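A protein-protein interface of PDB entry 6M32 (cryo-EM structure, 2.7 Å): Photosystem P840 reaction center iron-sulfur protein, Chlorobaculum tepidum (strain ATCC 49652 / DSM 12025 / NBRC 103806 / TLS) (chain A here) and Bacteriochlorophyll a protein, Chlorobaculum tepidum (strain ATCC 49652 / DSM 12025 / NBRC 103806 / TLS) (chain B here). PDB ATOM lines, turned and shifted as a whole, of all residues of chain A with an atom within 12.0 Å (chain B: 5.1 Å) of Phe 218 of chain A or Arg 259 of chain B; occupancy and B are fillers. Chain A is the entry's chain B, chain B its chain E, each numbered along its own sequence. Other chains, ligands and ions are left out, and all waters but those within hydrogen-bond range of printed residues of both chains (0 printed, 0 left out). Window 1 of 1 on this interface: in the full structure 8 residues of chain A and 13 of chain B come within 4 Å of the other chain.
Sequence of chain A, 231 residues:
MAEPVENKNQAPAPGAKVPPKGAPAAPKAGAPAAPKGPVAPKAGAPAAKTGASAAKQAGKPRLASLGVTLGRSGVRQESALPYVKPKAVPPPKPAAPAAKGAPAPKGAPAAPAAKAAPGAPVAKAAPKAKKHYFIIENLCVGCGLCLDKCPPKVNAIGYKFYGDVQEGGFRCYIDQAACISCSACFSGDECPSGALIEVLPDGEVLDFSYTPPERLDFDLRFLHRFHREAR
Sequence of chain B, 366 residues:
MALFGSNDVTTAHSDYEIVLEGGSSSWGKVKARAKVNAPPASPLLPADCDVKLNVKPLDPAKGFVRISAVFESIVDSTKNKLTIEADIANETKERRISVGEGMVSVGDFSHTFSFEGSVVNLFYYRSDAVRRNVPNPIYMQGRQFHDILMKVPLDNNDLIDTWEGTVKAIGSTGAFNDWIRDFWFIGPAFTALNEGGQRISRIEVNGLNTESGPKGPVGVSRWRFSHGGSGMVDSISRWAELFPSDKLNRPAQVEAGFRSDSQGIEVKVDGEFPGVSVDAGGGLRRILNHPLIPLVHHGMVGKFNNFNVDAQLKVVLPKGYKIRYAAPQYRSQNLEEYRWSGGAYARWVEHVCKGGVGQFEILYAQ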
ATOM      1  N   PRO A 212       5.621 -13.780  -3.470  1.00  0.00           N
ATOM      2  CA  PRO A 212       5.022 -13.698  -2.128  1.00  0.00           C
ATOM      3  C   PRO A 212       5.974 -13.049  -1.139  1.00  0.00           C
ATOM      4  O   PRO A 212       7.180 -12.961  -1.402  1.00  0.00           O
ATOM      5  CB  PRO A 212       4.764 -15.170  -1.779  1.00  0.00           C
ATOM      6  CG  PRO A 212       4.543 -15.815  -3.099  1.00  0.00           C
ATOM      7  CD  PRO A 212       5.480 -15.124  -4.054  1.00  0.00           C
ATOM      8  N   PRO A 213       5.470 -12.579   0.020  1.00  0.00           N
ATOM      9  CA  PRO A 213       6.265 -11.668   0.864  1.00  0.00           C
ATOM     10  C   PRO A 213       7.242 -12.296   1.859  1.00  0.00           C
ATOM     11  O   PRO A 213       7.672 -11.605   2.787  1.00  0.00           O
ATOM     12  CB  PRO A 213       5.182 -10.869   1.599  1.00  0.00           C
ATOM     13  CG  PRO A 213       4.033 -11.803   1.693  1.00  0.00           C
ATOM     14  CD  PRO A 213       4.067 -12.666   0.467  1.00  0.00           C
ATOM     15  N   GLU A 214       7.602 -13.572   1.689  1.00  0.00           N
ATOM     16  CA  GLU A 214       8.622 -14.281   2.485  1.00  0.00           C
ATOM     17  C   GLU A 214       8.505 -13.991   3.986  1.00  0.00           C
ATOM     18  O   GLU A 214       9.335 -13.320   4.599  1.00  0.00           O
ATOM     19  CB  GLU A 214      10.075 -14.068   2.012  1.00  0.00           C
ATOM     20  CG  GLU A 214      10.670 -12.668   1.856  1.00  0.00           C
ATOM     21  CD  GLU A 214      10.118 -11.907   0.673  1.00  0.00           C
ATOM     22  OE1 GLU A 214       9.329 -12.493  -0.087  1.00  0.00           O
ATOM     23  OE2 GLU A 214      10.497 -10.735   0.481  1.00  0.00           O
ATOM     24  N   ARG A 215       7.437 -14.524   4.560  1.00  0.00           N
ATOM     25  CA  ARG A 215       7.313 -14.648   6.002  1.00  0.00           C
ATOM     26  C   ARG A 215       8.193 -15.792   6.516  1.00  0.00           C
ATOM     27  O   ARG A 215       9.011 -16.355   5.785  1.00  0.00           O
ATOM     28  CB  ARG A 215       5.851 -14.871   6.356  1.00  0.00           C
ATOM     29  CG  ARG A 215       4.890 -14.036   5.535  1.00  0.00           C
ATOM     30  CD  ARG A 215       3.503 -14.482   5.866  1.00  0.00           C
ATOM     31  NE  ARG A 215       3.130 -14.025   7.193  1.00  0.00           N
ATOM     32  CZ  ARG A 215       3.014 -14.844   8.233  1.00  0.00           C
ATOM     33  NH1 ARG A 215       3.257 -16.139   8.086  1.00  0.00           N
ATOM     34  NH2 ARG A 215       2.669 -14.369   9.419  1.00  0.00           N
ATOM     35  N   LEU A 216       8.032 -16.142   7.796  1.00  0.00           N
ATOM     36  CA  LEU A 216       8.725 -17.279   8.395  1.00  0.00           C
ATOM     37  C   LEU A 216       7.861 -17.848   9.516  1.00  0.00           C
ATOM     38  O   LEU A 216       7.053 -17.133  10.105  1.00  0.00           O
ATOM     39  CB  LEU A 216      10.129 -16.878   8.895  1.00  0.00           C
ATOM     40  CG  LEU A 216      10.381 -15.902  10.047  1.00  0.00           C
ATOM     41  CD1 LEU A 216      10.429 -16.638  11.362  1.00  0.00           C
ATOM     42  CD2 LEU A 216      11.672 -15.148   9.839  1.00  0.00           C
ATOM     43  N   ASP A 217       8.052 -19.137   9.823  1.00  0.00           N
ATOM     44  CA  ASP A 217       6.971 -19.977  10.332  1.00  0.00           C
ATOM     45  C   ASP A 217       7.415 -20.809  11.539  1.00  0.00           C
ATOM     46  O   ASP A 217       8.612 -20.954  11.800  1.00  0.00           O
ATOM     47  CB  ASP A 217       6.485 -20.882   9.173  1.00  0.00           C
ATOM     48  CG  ASP A 217       5.732 -20.136   8.106  1.00  0.00           C
ATOM     49  OD1 ASP A 217       5.321 -18.983   8.357  1.00  0.00           O
ATOM     50  OD2 ASP A 217       5.493 -20.731   7.038  1.00  0.00           O
ATOM     51  N   PHE A 218       6.432 -21.343  12.283  1.00  0.00           N
ATOM     52  CA  PHE A 218       6.667 -22.339  13.331  1.00  0.00           C
ATOM     53  C   PHE A 218       5.472 -23.284  13.431  1.00  0.00           C
ATOM     54  O   PHE A 218       4.646 -23.382  12.522  1.00  0.00           O
ATOM     55  CB  PHE A 218       6.912 -21.727  14.721  1.00  0.00           C
ATOM     56  CG  PHE A 218       5.822 -20.800  15.204  1.00  0.00           C
ATOM     57  CD1 PHE A 218       6.069 -19.464  15.336  1.00  0.00           C
ATOM     58  CD2 PHE A 218       4.574 -21.268  15.578  1.00  0.00           C
ATOM     59  CE1 PHE A 218       5.096 -18.593  15.791  1.00  0.00           C
ATOM     60  CE2 PHE A 218       3.596 -20.404  16.033  1.00  0.00           C
ATOM     61  CZ  PHE A 218       3.864 -19.061  16.140  1.00  0.00           C
ATOM     62  N   ASP A 219       5.397 -23.994  14.561  1.00  0.00           N
ATOM     63  CA  ASP A 219       4.272 -24.861  14.887  1.00  0.00           C
ATOM     64  C   ASP A 219       3.566 -24.387  16.153  1.00  0.00           C
ATOM     65  O   ASP A 219       4.189 -23.832  17.063  1.00  0.00           O
ATOM     66  CB  ASP A 219       4.722 -26.315  15.079  1.00  0.00           C
ATOM     67  CG  ASP A 219       3.562 -27.248  15.372  1.00  0.00           C
ATOM     68  OD1 ASP A 219       2.805 -27.577  14.435  1.00  0.00           O
ATOM     69  OD2 ASP A 219       3.398 -27.642  16.546  1.00  0.00           O
ATOM     70  N   LEU A 220       2.257 -24.631  16.209  1.00  0.00           N
ATOM     71  CA  LEU A 220       1.421 -24.262  17.341  1.00  0.00           C
ATOM     72  C   LEU A 220       0.705 -25.490  17.892  1.00  0.00           C
ATOM     73  O   LEU A 220       0.492 -26.482  17.189  1.00  0.00           O
ATOM     74  CB  LEU A 220       0.396 -23.188  16.938  1.00  0.00           C
ATOM     75  CG  LEU A 220      -0.649 -23.505  15.865  1.00  0.00           C
ATOM     76  CD1 LEU A 220      -1.794 -24.306  16.456  1.00  0.00           C
ATOM     77  CD2 LEU A 220      -1.175 -22.236  15.221  1.00  0.00           C
ATOM     78  N   ARG A 221       0.341 -25.414  19.176  1.00  0.00           N
ATOM     79  CA  ARG A 221      -0.524 -26.416  19.803  1.00  0.00           C
ATOM     80  C   ARG A 221      -1.365 -25.704  20.861  1.00  0.00           C
ATOM     81  O   ARG A 221      -0.844 -25.321  21.912  1.00  0.00           O
ATOM     82  CB  ARG A 221       0.286 -27.551  20.413  1.00  0.00           C
ATOM     83  CG  ARG A 221       0.474 -28.752  19.502  1.00  0.00           C
ATOM     84  CD  ARG A 221       1.656 -29.599  19.939  1.00  0.00           C
ATOM     85  NE  ARG A 221       2.351 -30.184  18.796  1.00  0.00           N
ATOM     86  CZ  ARG A 221       3.348 -31.058  18.892  1.00  0.00           C
ATOM     87  NH1 ARG A 221       3.774 -31.454  20.084  1.00  0.00           N
ATOM     88  NH2 ARG A 221       3.918 -31.536  17.795  1.00  0.00           N
ATOM     89  N   PHE A 222      -2.657 -25.530  20.578  1.00  0.00           N
ATOM     90  CA  PHE A 222      -3.575 -25.001  21.581  1.00  0.00           C
ATOM     91  C   PHE A 222      -3.704 -25.955  22.758  1.00  0.00           C
ATOM     92  O   PHE A 222      -4.243 -27.057  22.614  1.00  0.00           O
ATOM     93  CB  PHE A 222      -4.962 -24.742  20.990  1.00  0.00           C
ATOM     94  CG  PHE A 222      -5.026 -23.560  20.075  1.00  0.00           C
ATOM     95  CD1 PHE A 222      -4.926 -22.276  20.581  1.00  0.00           C
ATOM     96  CD2 PHE A 222      -5.221 -23.729  18.716  1.00  0.00           C
ATOM     97  CE1 PHE A 222      -4.996 -21.186  19.749  1.00  0.00           C
ATOM     98  CE2 PHE A 222      -5.293 -22.638  17.878  1.00  0.00           C
ATOM     99  CZ  PHE A 222      -5.177 -21.367  18.400  1.00  0.00           C
ATOM    100  N   LEU A 223      -3.225 -25.541  23.924  1.00  0.00           N
ATOM    101  CA  LEU A 223      -3.368 -26.351  25.127  1.00  0.00           C
ATOM    102  C   LEU A 223      -4.698 -26.058  25.814  1.00  0.00           C
ATOM    103  O   LEU A 223      -4.955 -26.533  26.920  1.00  0.00           O
ATOM    104  CB  LEU A 223      -2.210 -26.103  26.098  1.00  0.00           C
ATOM    105  CG  LEU A 223      -2.156 -24.782  26.870  1.00  0.00           C
ATOM    106  CD1 LEU A 223      -1.176 -24.907  28.020  1.00  0.00           C
ATOM    107  CD2 LEU A 223      -1.758 -23.620  25.972  1.00  0.00           C
ATOM    108  N   ALA B  47       3.955  -8.759   9.192  1.00  0.00           N
ATOM    109  CA  ALA B  47       5.019  -8.477  10.147  1.00  0.00           C
ATOM    110  C   ALA B  47       5.146  -9.643  11.114  1.00  0.00           C
ATOM    111  O   ALA B  47       4.150 -10.068  11.703  1.00  0.00           O
ATOM    112  CB  ALA B  47       4.743  -7.177  10.904  1.00  0.00           C
ATOM    113  N   ASP B  48       6.366 -10.147  11.277  1.00  0.00           N
ATOM    114  CA  ASP B  48       6.659 -11.289  12.131  1.00  0.00           C
ATOM    115  C   ASP B  48       7.775 -10.916  13.101  1.00  0.00           C
ATOM    116  O   ASP B  48       8.608 -10.062  12.798  1.00  0.00           O
ATOM    117  CB  ASP B  48       7.082 -12.499  11.291  1.00  0.00           C
ATOM    118  CG  ASP B  48       6.158 -12.743  10.111  1.00  0.00           C
ATOM    119  OD1 ASP B  48       4.951 -12.454  10.222  1.00  0.00           O
ATOM    120  OD2 ASP B  48       6.638 -13.238   9.071  1.00  0.00           O
ATOM    121  N   CYS B  49       7.803 -11.556  14.272  1.00  0.00           N
ATOM    122  CA  CYS B  49       8.865 -11.273  15.230  1.00  0.00           C
ATOM    123  C   CYS B  49       9.004 -12.407  16.235  1.00  0.00           C
ATOM    124  O   CYS B  49       8.022 -13.021  16.654  1.00  0.00           O
ATOM    125  CB  CYS B  49       8.628  -9.952  15.964  1.00  0.00           C
ATOM    126  SG  CYS B  49       9.993  -9.433  17.026  1.00  0.00           S
ATOM    127  N   GLY B 257       6.948 -14.688  20.601  1.00  0.00           N
ATOM    128  CA  GLY B 257       6.904 -14.509  19.172  1.00  0.00           C
ATOM    129  C   GLY B 257       5.499 -14.246  18.687  1.00  0.00           C
ATOM    130  O   GLY B 257       4.556 -14.973  19.024  1.00  0.00           O
ATOM    131  N   PHE B 258       5.354 -13.204  17.883  1.00  0.00           N
ATOM    132  CA  PHE B 258       4.082 -12.918  17.246  1.00  0.00           C
ATOM    133  C   PHE B 258       4.296 -12.973  15.746  1.00  0.00           C
ATOM    134  O   PHE B 258       5.422 -12.887  15.251  1.00  0.00           O
ATOM    135  CB  PHE B 258       3.499 -11.561  17.667  1.00  0.00           C
ATOM    136  CG  PHE B 258       4.159 -10.378  17.022  1.00  0.00           C
ATOM    137  CD1 PHE B 258       3.713  -9.903  15.798  1.00  0.00           C
ATOM    138  CD2 PHE B 258       5.196  -9.717  17.649  1.00  0.00           C
ATOM    139  CE1 PHE B 258       4.305  -8.817  15.206  1.00  0.00           C
ATOM    140  CE2 PHE B 258       5.785  -8.620  17.064  1.00  0.00           C
ATOM    141  CZ  PHE B 258       5.344  -8.173  15.839  1.00  0.00           C
ATOM    142  N   ARG B 259       3.209 -13.210  15.029  1.00  0.00           N
ATOM    143  CA  ARG B 259       3.244 -13.298  13.583  1.00  0.00           C
ATOM    144  C   ARG B 259       1.936 -12.705  13.106  1.00  0.00           C
ATOM    145  O   ARG B 259       0.870 -13.287  13.281  1.00  0.00           O
ATOM    146  CB  ARG B 259       3.428 -14.749  13.139  1.00  0.00           C
ATOM    147  CG  ARG B 259       2.322 -15.706  13.543  1.00  0.00           C
ATOM    148  CD  ARG B 259       2.626 -17.107  13.043  1.00  0.00           C
ATOM    149  NE  ARG B 259       2.627 -17.172  11.586  1.00  0.00           N
ATOM    150  CZ  ARG B 259       2.956 -18.254  10.890  1.00  0.00           C
ATOM    151  NH1 ARG B 259       2.928 -18.228   9.567  1.00  0.00           N
ATOM    152  NH2 ARG B 259       3.315 -19.362  11.520  1.00  0.00           N
ATOM    153  N   SER B 260       2.025 -11.518  12.526  1.00  0.00           N
ATOM    154  CA  SER B 260       0.848 -10.797  12.073  1.00  0.00           C
ATOM    155  C   SER B 260       0.734 -10.844  10.560  1.00  0.00           C
ATOM    156  O   SER B 260       1.679 -11.186   9.849  1.00  0.00           O
ATOM    157  CB  SER B 260       0.882  -9.342  12.545  1.00  0.00           C
ATOM    158  OG  SER B 260       0.803  -9.265  13.956  1.00  0.00           O
ATOM    159  N   ASP B 261      -0.431 -10.435  10.076  1.00  0.00           N
ATOM    160  CA  ASP B 261      -0.856 -10.683   8.708  1.00  0.00           C
ATOM    161  C   ASP B 261      -2.086  -9.826   8.453  1.00  0.00           C
ATOM    162  O   ASP B 261      -2.590  -9.165   9.359  1.00  0.00           O
ATOM    163  CB  ASP B 261      -1.185 -12.162   8.492  1.00  0.00           C
ATOM    164  CG  ASP B 261       0.033 -13.048   8.495  1.00  0.00           C
ATOM    165  OD1 ASP B 261       1.166 -12.547   8.380  1.00  0.00           O
ATOM    166  OD2 ASP B 261      -0.139 -14.275   8.612  1.00  0.00           O
ATOM    167  N   GLY B 264      -5.596 -11.240  10.971  1.00  0.00           N
ATOM    168  CA  GLY B 264      -5.653 -11.720  12.333  1.00  0.00           C
ATOM    169  C   GLY B 264      -4.230 -11.801  12.850  1.00  0.00           C
ATOM    170  O   GLY B 264      -3.276 -11.575  12.104  1.00  0.00           O
ATOM    171  N   ILE B 265      -4.093 -12.134  14.129  1.00  0.00           N
ATOM    172  CA  ILE B 265      -2.800 -12.107  14.792  1.00  0.00           C
ATOM    173  C   ILE B 265      -2.586 -13.392  15.575  1.00  0.00           C
ATOM    174  O   ILE B 265      -3.496 -13.920  16.222  1.00  0.00           O
ATOM    175  CB  ILE B 265      -2.654 -10.876  15.704  1.00  0.00           C
ATOM    176  CG1 ILE B 265      -3.025  -9.619  14.919  1.00  0.00           C
ATOM    177  CG2 ILE B 265      -1.254 -10.777  16.263  1.00  0.00           C
ATOM    178  CD1 ILE B 265      -3.267  -8.436  15.761  1.00  0.00           C
ATOM    179  N   GLU B 266      -1.344 -13.872  15.511  1.00  0.00           N
ATOM    180  CA  GLU B 266      -0.882 -15.090  16.160  1.00  0.00           C
ATOM    181  C   GLU B 266       0.121 -14.741  17.251  1.00  0.00           C
ATOM    182  O   GLU B 266       0.988 -13.886  17.052  1.00  0.00           O
ATOM    183  CB  GLU B 266      -0.224 -16.019  15.136  1.00  0.00           C
ATOM    184  CG  GLU B 266       0.253 -17.373  15.643  1.00  0.00           C
ATOM    185  CD  GLU B 266      -0.861 -18.291  16.119  1.00  0.00           C
ATOM    186  OE1 GLU B 266      -2.051 -18.019  15.854  1.00  0.00           O
ATOM    187  OE2 GLU B 266      -0.542 -19.304  16.771  1.00  0.00           O
ATOM    188  N   LYS B 268       2.594 -16.449  20.653  1.00  0.00           N
ATOM    189  CA  LYS B 268       3.143 -17.632  21.307  1.00  0.00           C
ATOM    190  C   LYS B 268       4.197 -17.194  22.314  1.00  0.00           C
ATOM    191  O   LYS B 268       5.162 -16.529  21.935  1.00  0.00           O
ATOM    192  CB  LYS B 268       3.752 -18.576  20.269  1.00  0.00           C
ATOM    193  CG  LYS B 268       4.339 -19.845  20.847  1.00  0.00           C
ATOM    194  CD  LYS B 268       4.927 -20.740  19.769  1.00  0.00           C
ATOM    195  CE  LYS B 268       5.976 -20.006  18.942  1.00  0.00           C
ATOM    196  NZ  LYS B 268       6.944 -19.231  19.772  1.00  0.00           N
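The guanidinium group (NH2) of Arg 215 of chain A is in salt-bridge range of the side-chain carboxylate (OD1) of Asp 48 of chain B, 3.1 Å away.
The side-chain carboxylate (OD2) of Asp 48 of chain B sits at hydrogen-bond distance from the backbone NH (N) of Leu 216 of chain A, 3.5 Å away.
The guanidinium group of Arg 259 of chain B lies close to the guanidinium group of Arg 215 of chain A (2.6 Å).
OD1 of Asp 217 of chain A is in salt-bridge range of NH1 of Arg 259 of chain B, at 2.8 Å.
O of Ser 260 of chain B sits at hydrogen-bond distance from NH2 of Arg 215 of chain A (3.4 Å).
The side-chain carboxylate (OD1) of Asp 261 of chain B is in salt-bridge range of the guanidinium group (NH2) of Arg 215 of chain A (2.6 Å).
The backbone carbonyl oxygen (O) of Ala 47 of chain B lies within hydrogen-bond range of the backbone NH (N) of Ser 260 of chain B.
O of Lys 268 of chain B is in hydrogen-bond range of N of Gly 257 of chain B, at 2.9 Å.
The backbone NH (N) of Arg 259 of chain B lies within hydrogen-bond range of the backbone carbonyl oxygen (O) of Glu 266 of chain B (3.1 Å).
OD1 of Asp 217 of chain A lies within salt-bridge range of NH1 of Arg 215 of chain A.
Among the printed residues, pairs that only touch across the chains: Phe 218 of chain A with Arg 259 of chain B (3.8 Å), Phe 218 of chain A with Lys 268 of chain B (3.6 Å) and Leu 220 of chain A with Glu 266 of chain B (3.4 Å).
Printed residues of chain B within 4 Å of Phe 218 of chain A: Arg 259 (3.8 Å) and Lys 268 (3.6 Å).
No residue of chain A comes within 4 Å of Ala 47 of chain B.
Of chain A, only Arg 215 and Leu 216 come within 4 Å of Asp 48 of chain B.
No residue of chain A comes within 4 Å of Gly 257 of chain B.
Ser 260 of chain B touches one residue of chain A.
Asp 261 of chain B touches just one residue of chain A: Arg 215 (2.6 Å).
No residue of chain A comes within 4 Å of Gly 264 of chain B.
No residue of chain A comes within 4 Å of Ile 265 of chain B.
Lys 268 of chain B touches one residue of chain A.
Of the printed residues of chain B, Leu 220 of chain A touches Glu 266 (3.4 Å).
Printed residues of chain B within 4 Å of Asp 217 of chain A: Arg 259.
Glu 214 of chain A touches none of the printed residues of chain B.
Cys 49 of chain B touches none of the printed residues of chain A.
The nearest residue of chain A that does not touch Arg 259 of chain B is Leu 216 of chain A (4.3 Å).
Printed residues of chain A that touch a printed residue of chain B: Arg 215, Leu 216, Asp 217, Phe 218 and Leu 220.
Along chain A the printed residues that touch a printed residue of chain B span positions 215 to 220.
Among the printed residues, Asp or Glu carboxylates within 4 Å of a Lys or Arg side-chain nitrogen of the other chain: Arg 215 of chain A with Asp 48 of chain B (3.1 Å), Arg 215 of chain A with Asp 261 of chain B (2.6 Å) and Asp 217 of chain A with Arg 259 of chain B (2.8 Å).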
